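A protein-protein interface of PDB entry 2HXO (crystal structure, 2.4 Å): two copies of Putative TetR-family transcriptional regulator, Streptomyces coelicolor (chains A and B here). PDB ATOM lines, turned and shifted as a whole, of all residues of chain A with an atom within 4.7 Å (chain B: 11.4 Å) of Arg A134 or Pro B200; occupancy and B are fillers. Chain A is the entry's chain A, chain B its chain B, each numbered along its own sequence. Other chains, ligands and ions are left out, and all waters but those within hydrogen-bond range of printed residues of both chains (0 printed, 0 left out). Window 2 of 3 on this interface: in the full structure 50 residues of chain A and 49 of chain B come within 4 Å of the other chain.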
ATOM      1  N   GLU A 130       9.592 -27.659  10.563  1.00  0.00           N
ATOM      2  CA  GLU A 130       8.772 -27.710   9.358  1.00  0.00           C
ATOM      3  C   GLU A 130       9.530 -28.503   8.284  1.00  0.00           C
ATOM      4  O   GLU A 130       8.954 -29.319   7.589  1.00  0.00           O
ATOM      5  CB  GLU A 130       8.488 -26.295   8.854  1.00  0.00           C
ATOM      6  CG  GLU A 130       7.520 -26.205   7.683  1.00  0.00           C
ATOM      7  CD  GLU A 130       6.089 -26.598   8.040  1.00  0.00           C
ATOM      8  OE1 GLU A 130       5.691 -26.457   9.206  1.00  0.00           O
ATOM      9  OE2 GLU A 130       5.349 -27.028   7.139  1.00  0.00           O
ATOM     10  N   SER A 131      10.827 -28.250   8.167  1.00  0.00           N
ATOM     11  CA  SER A 131      11.671 -28.927   7.192  1.00  0.00           C
ATOM     12  C   SER A 131      11.683 -30.439   7.412  1.00  0.00           C
ATOM     13  O   SER A 131      11.516 -31.204   6.464  1.00  0.00           O
ATOM     14  CB  SER A 131      13.106 -28.403   7.282  1.00  0.00           C
ATOM     15  OG  SER A 131      13.158 -27.008   7.060  1.00  0.00           O
ATOM     16  N   LEU A 132      11.896 -30.865   8.654  1.00  0.00           N
ATOM     17  CA  LEU A 132      11.930 -32.283   8.978  1.00  0.00           C
ATOM     18  C   LEU A 132      10.538 -32.914   8.877  1.00  0.00           C
ATOM     19  O   LEU A 132      10.379 -33.982   8.275  1.00  0.00           O
ATOM     20  CB  LEU A 132      12.503 -32.487  10.381  1.00  0.00           C
ATOM     21  CG  LEU A 132      13.916 -31.933  10.624  1.00  0.00           C
ATOM     22  CD1 LEU A 132      14.269 -32.040  12.117  1.00  0.00           C
ATOM     23  CD2 LEU A 132      14.918 -32.682   9.780  1.00  0.00           C
ATOM     24  N   GLY A 133       9.541 -32.243   9.451  1.00  0.00           N
ATOM     25  CA  GLY A 133       8.177 -32.753   9.447  1.00  0.00           C
ATOM     26  C   GLY A 133       7.588 -33.144   8.096  1.00  0.00           C
ATOM     27  O   GLY A 133       7.003 -34.227   7.949  1.00  0.00           O
ATOM     28  N   ARG A 134       7.735 -32.263   7.104  1.00  0.00           N
ATOM     29  CA  ARG A 134       7.212 -32.533   5.767  1.00  0.00           C
ATOM     30  C   ARG A 134       7.770 -33.832   5.203  1.00  0.00           C
ATOM     31  O   ARG A 134       7.071 -34.552   4.493  1.00  0.00           O
ATOM     32  CB  ARG A 134       7.542 -31.380   4.805  1.00  0.00           C
ATOM     33  CG  ARG A 134       6.794 -30.082   5.102  1.00  0.00           C
ATOM     34  CD  ARG A 134       7.065 -29.030   4.039  1.00  0.00           C
ATOM     35  NE  ARG A 134       6.541 -27.723   4.422  1.00  0.00           N
ATOM     36  CZ  ARG A 134       6.593 -26.646   3.645  1.00  0.00           C
ATOM     37  NH1 ARG A 134       7.143 -26.725   2.434  1.00  0.00           N
ATOM     38  NH2 ARG A 134       6.110 -25.484   4.083  1.00  0.00           N
ATOM     39  N   GLN A 135       9.029 -34.126   5.517  1.00  0.00           N
ATOM     40  CA  GLN A 135       9.658 -35.345   5.042  1.00  0.00           C
ATOM     41  C   GLN A 135       9.107 -36.555   5.797  1.00  0.00           C
ATOM     42  O   GLN A 135       8.923 -37.619   5.219  1.00  0.00           O
ATOM     43  CB  GLN A 135      11.177 -35.232   5.187  1.00  0.00           C
ATOM     44  CG  GLN A 135      11.769 -34.018   4.424  1.00  0.00           C
ATOM     45  CD  GLN A 135      11.259 -33.908   2.974  1.00  0.00           C
ATOM     46  OE1 GLN A 135      11.096 -34.906   2.277  1.00  0.00           O
ATOM     47  NE2 GLN A 135      11.013 -32.689   2.530  1.00  0.00           N
ATOM     48  N   VAL A 136       8.823 -36.376   7.081  1.00  0.00           N
ATOM     49  CA  VAL A 136       8.259 -37.432   7.910  1.00  0.00           C
ATOM     50  C   VAL A 136       6.881 -37.790   7.361  1.00  0.00           C
ATOM     51  O   VAL A 136       6.525 -38.961   7.259  1.00  0.00           O
ATOM     52  CB  VAL A 136       8.146 -36.970   9.386  1.00  0.00           C
ATOM     53  CG1 VAL A 136       7.214 -37.868  10.154  1.00  0.00           C
ATOM     54  CG2 VAL A 136       9.529 -36.976  10.024  1.00  0.00           C
ATOM     55  N   GLN A 137       6.103 -36.781   7.005  1.00  0.00           N
ATOM     56  CA  GLN A 137       4.784 -37.032   6.431  1.00  0.00           C
ATOM     57  C   GLN A 137       4.948 -37.742   5.079  1.00  0.00           C
ATOM     58  O   GLN A 137       4.234 -38.690   4.781  1.00  0.00           O
ATOM     59  CB  GLN A 137       4.022 -35.722   6.205  1.00  0.00           C
ATOM     60  CG  GLN A 137       3.863 -34.851   7.425  1.00  0.00           C
ATOM     61  CD  GLN A 137       3.031 -33.613   7.141  1.00  0.00           C
ATOM     62  OE1 GLN A 137       3.407 -32.768   6.333  1.00  0.00           O
ATOM     63  NE2 GLN A 137       1.882 -33.507   7.804  1.00  0.00           N
ATOM     64  N   ALA A 138       5.898 -37.295   4.268  1.00  0.00           N
ATOM     65  CA  ALA A 138       6.108 -37.924   2.963  1.00  0.00           C
ATOM     66  C   ALA A 138       6.504 -39.396   3.137  1.00  0.00           C
ATOM     67  O   ALA A 138       6.278 -40.220   2.256  1.00  0.00           O
ATOM     68  CB  ALA A 138       7.188 -37.170   2.181  1.00  0.00           C
ATOM     69  N   TRP B 191       3.188 -21.386  17.966  1.00  0.00           N
ATOM     70  CA  TRP B 191       3.150 -22.136  16.714  1.00  0.00           C
ATOM     71  C   TRP B 191       1.750 -22.126  16.110  1.00  0.00           C
ATOM     72  O   TRP B 191       1.600 -22.158  14.890  1.00  0.00           O
ATOM     73  CB  TRP B 191       3.646 -23.577  16.934  1.00  0.00           C
ATOM     74  CG  TRP B 191       5.143 -23.670  17.146  1.00  0.00           C
ATOM     75  CD1 TRP B 191       5.989 -22.643  17.456  1.00  0.00           C
ATOM     76  CD2 TRP B 191       5.949 -24.860  17.124  1.00  0.00           C
ATOM     77  NE1 TRP B 191       7.265 -23.116  17.634  1.00  0.00           N
ATOM     78  CE2 TRP B 191       7.272 -24.472  17.438  1.00  0.00           C
ATOM     79  CE3 TRP B 191       5.683 -26.215  16.877  1.00  0.00           C
ATOM     80  CZ2 TRP B 191       8.329 -25.391  17.512  1.00  0.00           C
ATOM     81  CZ3 TRP B 191       6.738 -27.135  16.954  1.00  0.00           C
ATOM     82  CH2 TRP B 191       8.043 -26.714  17.270  1.00  0.00           C
ATOM     83  N   GLU B 192       0.721 -22.077  16.952  1.00  0.00           N
ATOM     84  CA  GLU B 192      -0.644 -22.031  16.427  1.00  0.00           C
ATOM     85  C   GLU B 192      -0.887 -20.686  15.752  1.00  0.00           C
ATOM     86  O   GLU B 192      -1.865 -20.511  15.028  1.00  0.00           O
ATOM     87  CB  GLU B 192      -1.673 -22.281  17.541  1.00  0.00           C
ATOM     88  CG  GLU B 192      -1.623 -23.721  18.043  1.00  0.00           C
ATOM     89  CD  GLU B 192      -2.626 -24.044  19.140  1.00  0.00           C
ATOM     90  OE1 GLU B 192      -2.637 -23.338  20.179  1.00  0.00           O
ATOM     91  OE2 GLU B 192      -3.392 -25.023  18.960  1.00  0.00           O
ATOM     92  N   GLY B 193       0.029 -19.746  15.981  1.00  0.00           N
ATOM     93  CA  GLY B 193      -0.092 -18.434  15.368  1.00  0.00           C
ATOM     94  C   GLY B 193       0.658 -18.318  14.050  1.00  0.00           C
ATOM     95  O   GLY B 193       0.700 -17.252  13.448  1.00  0.00           O
ATOM     96  N   LEU B 194       1.257 -19.415  13.595  1.00  0.00           N
ATOM     97  CA  LEU B 194       2.010 -19.401  12.344  1.00  0.00           C
ATOM     98  C   LEU B 194       1.076 -19.555  11.147  1.00  0.00           C
ATOM     99  O   LEU B 194       0.029 -20.195  11.242  1.00  0.00           O
ATOM    100  CB  LEU B 194       3.053 -20.527  12.339  1.00  0.00           C
ATOM    101  CG  LEU B 194       4.270 -20.456  13.272  1.00  0.00           C
ATOM    102  CD1 LEU B 194       4.942 -21.835  13.333  1.00  0.00           C
ATOM    103  CD2 LEU B 194       5.249 -19.392  12.784  1.00  0.00           C
ATOM    104  N   ASP B 195       1.459 -18.967  10.021  1.00  0.00           N
ATOM    105  CA  ASP B 195       0.639 -19.050   8.818  1.00  0.00           C
ATOM    106  C   ASP B 195       0.430 -20.509   8.404  1.00  0.00           C
ATOM    107  O   ASP B 195       1.396 -21.238   8.143  1.00  0.00           O
ATOM    108  CB  ASP B 195       1.284 -18.266   7.670  1.00  0.00           C
ATOM    109  CG  ASP B 195       0.432 -18.276   6.416  1.00  0.00           C
ATOM    110  OD1 ASP B 195       0.620 -19.169   5.559  1.00  0.00           O
ATOM    111  OD2 ASP B 195      -0.444 -17.395   6.291  1.00  0.00           O
ATOM    112  N   PRO B 196      -0.847 -20.945   8.328  1.00  0.00           N
ATOM    113  CA  PRO B 196      -1.249 -22.310   7.955  1.00  0.00           C
ATOM    114  C   PRO B 196      -0.796 -22.774   6.579  1.00  0.00           C
ATOM    115  O   PRO B 196      -0.618 -23.972   6.357  1.00  0.00           O
ATOM    116  CB  PRO B 196      -2.776 -22.276   8.088  1.00  0.00           C
ATOM    117  CG  PRO B 196      -3.112 -20.836   7.781  1.00  0.00           C
ATOM    118  CD  PRO B 196      -2.033 -20.091   8.547  1.00  0.00           C
ATOM    119  N   ASP B 197      -0.614 -21.842   5.650  1.00  0.00           N
ATOM    120  CA  ASP B 197      -0.175 -22.222   4.316  1.00  0.00           C
ATOM    121  C   ASP B 197       1.344 -22.356   4.222  1.00  0.00           C
ATOM    122  O   ASP B 197       1.865 -23.153   3.435  1.00  0.00           O
ATOM    123  CB  ASP B 197      -0.669 -21.207   3.284  1.00  0.00           C
ATOM    124  CG  ASP B 197      -2.092 -21.485   2.825  1.00  0.00           C
ATOM    125  OD1 ASP B 197      -2.416 -21.127   1.672  1.00  0.00           O
ATOM    126  OD2 ASP B 197      -2.890 -22.056   3.605  1.00  0.00           O
ATOM    127  N   ALA B 198       2.049 -21.574   5.032  1.00  0.00           N
ATOM    128  CA  ALA B 198       3.502 -21.606   5.028  1.00  0.00           C
ATOM    129  C   ALA B 198       4.029 -22.724   5.919  1.00  0.00           C
ATOM    130  O   ALA B 198       5.052 -23.327   5.624  1.00  0.00           O
ATOM    131  CB  ALA B 198       4.066 -20.238   5.488  1.00  0.00           C
ATOM    132  N   TYR B 199       3.312 -23.000   7.003  1.00  0.00           N
ATOM    133  CA  TYR B 199       3.709 -24.038   7.946  1.00  0.00           C
ATOM    134  C   TYR B 199       2.607 -25.070   8.145  1.00  0.00           C
ATOM    135  O   TYR B 199       2.027 -25.162   9.231  1.00  0.00           O
ATOM    136  CB  TYR B 199       4.045 -23.438   9.311  1.00  0.00           C
ATOM    137  CG  TYR B 199       5.176 -22.450   9.322  1.00  0.00           C
ATOM    138  CD1 TYR B 199       4.962 -21.118   8.975  1.00  0.00           C
ATOM    139  CD2 TYR B 199       6.461 -22.837   9.722  1.00  0.00           C
ATOM    140  CE1 TYR B 199       6.002 -20.177   9.036  1.00  0.00           C
ATOM    141  CE2 TYR B 199       7.509 -21.914   9.782  1.00  0.00           C
ATOM    142  CZ  TYR B 199       7.272 -20.586   9.442  1.00  0.00           C
ATOM    143  OH  TYR B 199       8.281 -19.658   9.559  1.00  0.00           O
ATOM    144  N   PRO B 200       2.305 -25.865   7.104  1.00  0.00           N
ATOM    145  CA  PRO B 200       1.254 -26.884   7.229  1.00  0.00           C
ATOM    146  C   PRO B 200       1.603 -27.989   8.250  1.00  0.00           C
ATOM    147  O   PRO B 200       0.734 -28.469   8.979  1.00  0.00           O
ATOM    148  CB  PRO B 200       1.109 -27.404   5.798  1.00  0.00           C
ATOM    149  CG  PRO B 200       2.499 -27.222   5.229  1.00  0.00           C
ATOM    150  CD  PRO B 200       2.891 -25.865   5.750  1.00  0.00           C
ATOM    151  N   PHE B 201       2.874 -28.378   8.317  1.00  0.00           N
ATOM    152  CA  PHE B 201       3.266 -29.409   9.276  1.00  0.00           C
ATOM    153  C   PHE B 201       3.255 -28.880  10.709  1.00  0.00           C
ATOM    154  O   PHE B 201       2.608 -29.449  11.595  1.00  0.00           O
ATOM    155  CB  PHE B 201       4.670 -29.938   8.976  1.00  0.00           C
ATOM    156  CG  PHE B 201       5.198 -30.878  10.032  1.00  0.00           C
ATOM    157  CD1 PHE B 201       4.843 -32.230  10.029  1.00  0.00           C
ATOM    158  CD2 PHE B 201       6.015 -30.404  11.058  1.00  0.00           C
ATOM    159  CE1 PHE B 201       5.294 -33.097  11.035  1.00  0.00           C
ATOM    160  CE2 PHE B 201       6.472 -31.264  12.071  1.00  0.00           C
ATOM    161  CZ  PHE B 201       6.109 -32.611  12.055  1.00  0.00           C
ATOM    162  N   THR B 202       3.992 -27.796  10.934  1.00  0.00           N
ATOM    163  CA  THR B 202       4.103 -27.213  12.261  1.00  0.00           C
ATOM    164  C   THR B 202       2.755 -26.812  12.845  1.00  0.00           C
ATOM    165  O   THR B 202       2.543 -26.911  14.055  1.00  0.00           O
ATOM    166  CB  THR B 202       5.062 -26.006  12.251  1.00  0.00           C
ATOM    167  OG1 THR B 202       6.335 -26.421  11.752  1.00  0.00           O
ATOM    168  CG2 THR B 202       5.258 -25.462  13.653  1.00  0.00           C
ATOM    169  N   ARG B 203       1.837 -26.374  11.988  1.00  0.00           N
ATOM    170  CA  ARG B 203       0.508 -25.991  12.446  1.00  0.00           C
ATOM    171  C   ARG B 203      -0.254 -27.241  12.831  1.00  0.00           C
ATOM    172  O   ARG B 203      -0.967 -27.277  13.838  1.00  0.00           O
ATOM    173  CB  ARG B 203      -0.230 -25.228  11.346  1.00  0.00           C
ATOM    174  CG  ARG B 203       0.091 -23.748  11.349  1.00  0.00           C
ATOM    175  CD  ARG B 203      -0.521 -23.099  12.579  1.00  0.00           C
ATOM    176  NE  ARG B 203      -1.902 -22.684  12.333  1.00  0.00           N
ATOM    177  CZ  ARG B 203      -2.849 -22.625  13.265  1.00  0.00           C
ATOM    178  NH1 ARG B 203      -2.575 -22.964  14.518  1.00  0.00           N
ATOM    179  NH2 ARG B 203      -4.070 -22.217  12.943  1.00  0.00           N
ATOM    180  N   ALA B 204      -0.086 -28.279  12.025  1.00  0.00           N
ATOM    181  CA  ALA B 204      -0.741 -29.552  12.281  1.00  0.00           C
ATOM    182  C   ALA B 204      -0.278 -30.163  13.608  1.00  0.00           C
ATOM    183  O   ALA B 204      -1.069 -30.774  14.307  1.00  0.00           O
ATOM    184  CB  ALA B 204      -0.473 -30.514  11.120  1.00  0.00           C
ATOM    185  N   VAL B 205       0.994 -29.994  13.969  1.00  0.00           N
ATOM    186  CA  VAL B 205       1.489 -30.562  15.226  1.00  0.00           C
ATOM    187  C   VAL B 205       1.451 -29.626  16.452  1.00  0.00           C
ATOM    188  O   VAL B 205       1.507 -30.098  17.590  1.00  0.00           O
ATOM    189  CB  VAL B 205       2.957 -31.094  15.093  1.00  0.00           C
ATOM    190  CG1 VAL B 205       3.037 -32.160  13.997  1.00  0.00           C
ATOM    191  CG2 VAL B 205       3.930 -29.934  14.824  1.00  0.00           C
ATOM    192  N   ALA B 206       1.369 -28.319  16.216  1.00  0.00           N
ATOM    193  CA  ALA B 206       1.338 -27.329  17.292  1.00  0.00           C
ATOM    194  C   ALA B 206       0.565 -27.781  18.520  1.00  0.00           C
ATOM    195  O   ALA B 206       0.986 -27.570  19.651  1.00  0.00           O
ATOM    196  CB  ALA B 206       0.750 -26.024  16.774  1.00  0.00           C
ATOM    197  N   ASP B 207      -0.572 -28.411  18.289  1.00  0.00           N
ATOM    198  CA  ASP B 207      -1.409 -28.885  19.373  1.00  0.00           C
ATOM    199  C   ASP B 207      -0.686 -29.936  20.214  1.00  0.00           C
ATOM    200  O   ASP B 207      -0.765 -29.917  21.446  1.00  0.00           O
ATOM    201  CB  ASP B 207      -2.693 -29.477  18.788  1.00  0.00           C
ATOM    202  CG  ASP B 207      -3.843 -29.457  19.768  1.00  0.00           C
ATOM    203  OD1 ASP B 207      -4.849 -30.155  19.501  1.00  0.00           O
ATOM    204  OD2 ASP B 207      -3.751 -28.741  20.791  1.00  0.00           O
ATOM    205  N   GLN B 208       0.018 -30.845  19.537  1.00  0.00           N
ATOM    206  CA  GLN B 208       0.763 -31.931  20.181  1.00  0.00           C
ATOM    207  C   GLN B 208       1.888 -31.469  21.116  1.00  0.00           C
ATOM    208  O   GLN B 208       2.356 -32.239  21.958  1.00  0.00           O
ATOM    209  CB  GLN B 208       1.382 -32.855  19.129  1.00  0.00           C
ATOM    210  CG  GLN B 208       0.415 -33.677  18.303  1.00  0.00           C
ATOM    211  CD  GLN B 208       1.108 -34.860  17.624  1.00  0.00           C
ATOM    212  OE1 GLN B 208       1.959 -34.690  16.750  1.00  0.00           O
ATOM    213  NE2 GLN B 208       0.750 -36.070  18.043  1.00  0.00           N
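The side-chain carboxylate (OE2) of Glu A130 lies within hydrogen-bond range of the backbone NH (N) of Phe B201. OG1 of Thr B202 sits at hydrogen-bond distance from OE1 of Glu A130 (2.6 Å). NH2 of Arg A134 sits at hydrogen-bond distance from O of Ala B198. The side-chain carboxylate (OE2) of Glu A130 sits close to the backbone nitrogen (N) of Pro B200 (3.3 Å).
NE of Arg A134 is in salt-bridge range of OE2 of Glu A130, at 3.0 Å. OD1 of Asp B195 lies within hydrogen-bond range of N of Ala B198, at 2.8 Å.
Glu A130 touches Tyr B199 (OE1 to CA, 3.4 Å). Phe B201 touches Gly A133. Arg A134 touches Pro B200. Gln A137 touches Phe B201.
Arg A134 touches just these residues of chain B: Ala B198 and Pro B200. Of chain A, only Glu A130 and Arg A134 come within 4 Å of Pro B200. Of chain B, only Phe B201 comes within 4 Å of Gly A133. No residue of chain B comes within 4 Å of Val A136. Gln A137 touches one residue of chain B. No residue of chain B comes within 4 Å of Ala A138. Printed residues of chain A within 4 Å of Tyr B199: Glu A130 (3.4 Å). Of the printed residues of chain A, Phe B201 touches Glu A130 (3.1 Å), Gly A133 (3.3 Å) and Gln A137 (3.7 Å). Printed residues of chain A within 4 Å of Thr B202: Glu A130. Arg B203 touches none of the printed residues of chain A. The nearest residue of chain B that does not touch Arg A134 is Phe B201 (4.1 Å). The nearest printed residue of chain A that does not touch Pro B200 is Gln A137 (5.3 Å).
Of the 18 printed residues of chain B, 5 touch a printed residue of chain A. Along chain B the printed residues that touch a printed residue of chain A span positions 198 to 202. Printed residues of chain A that touch a printed residue of chain B: Glu A130, Gly A133, Arg A134 and Gln A137.
No position is printed for both chains. Of the 8 pairs that touch across the chains among the printed residues, none has its exchanged pair printed and touching as well.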
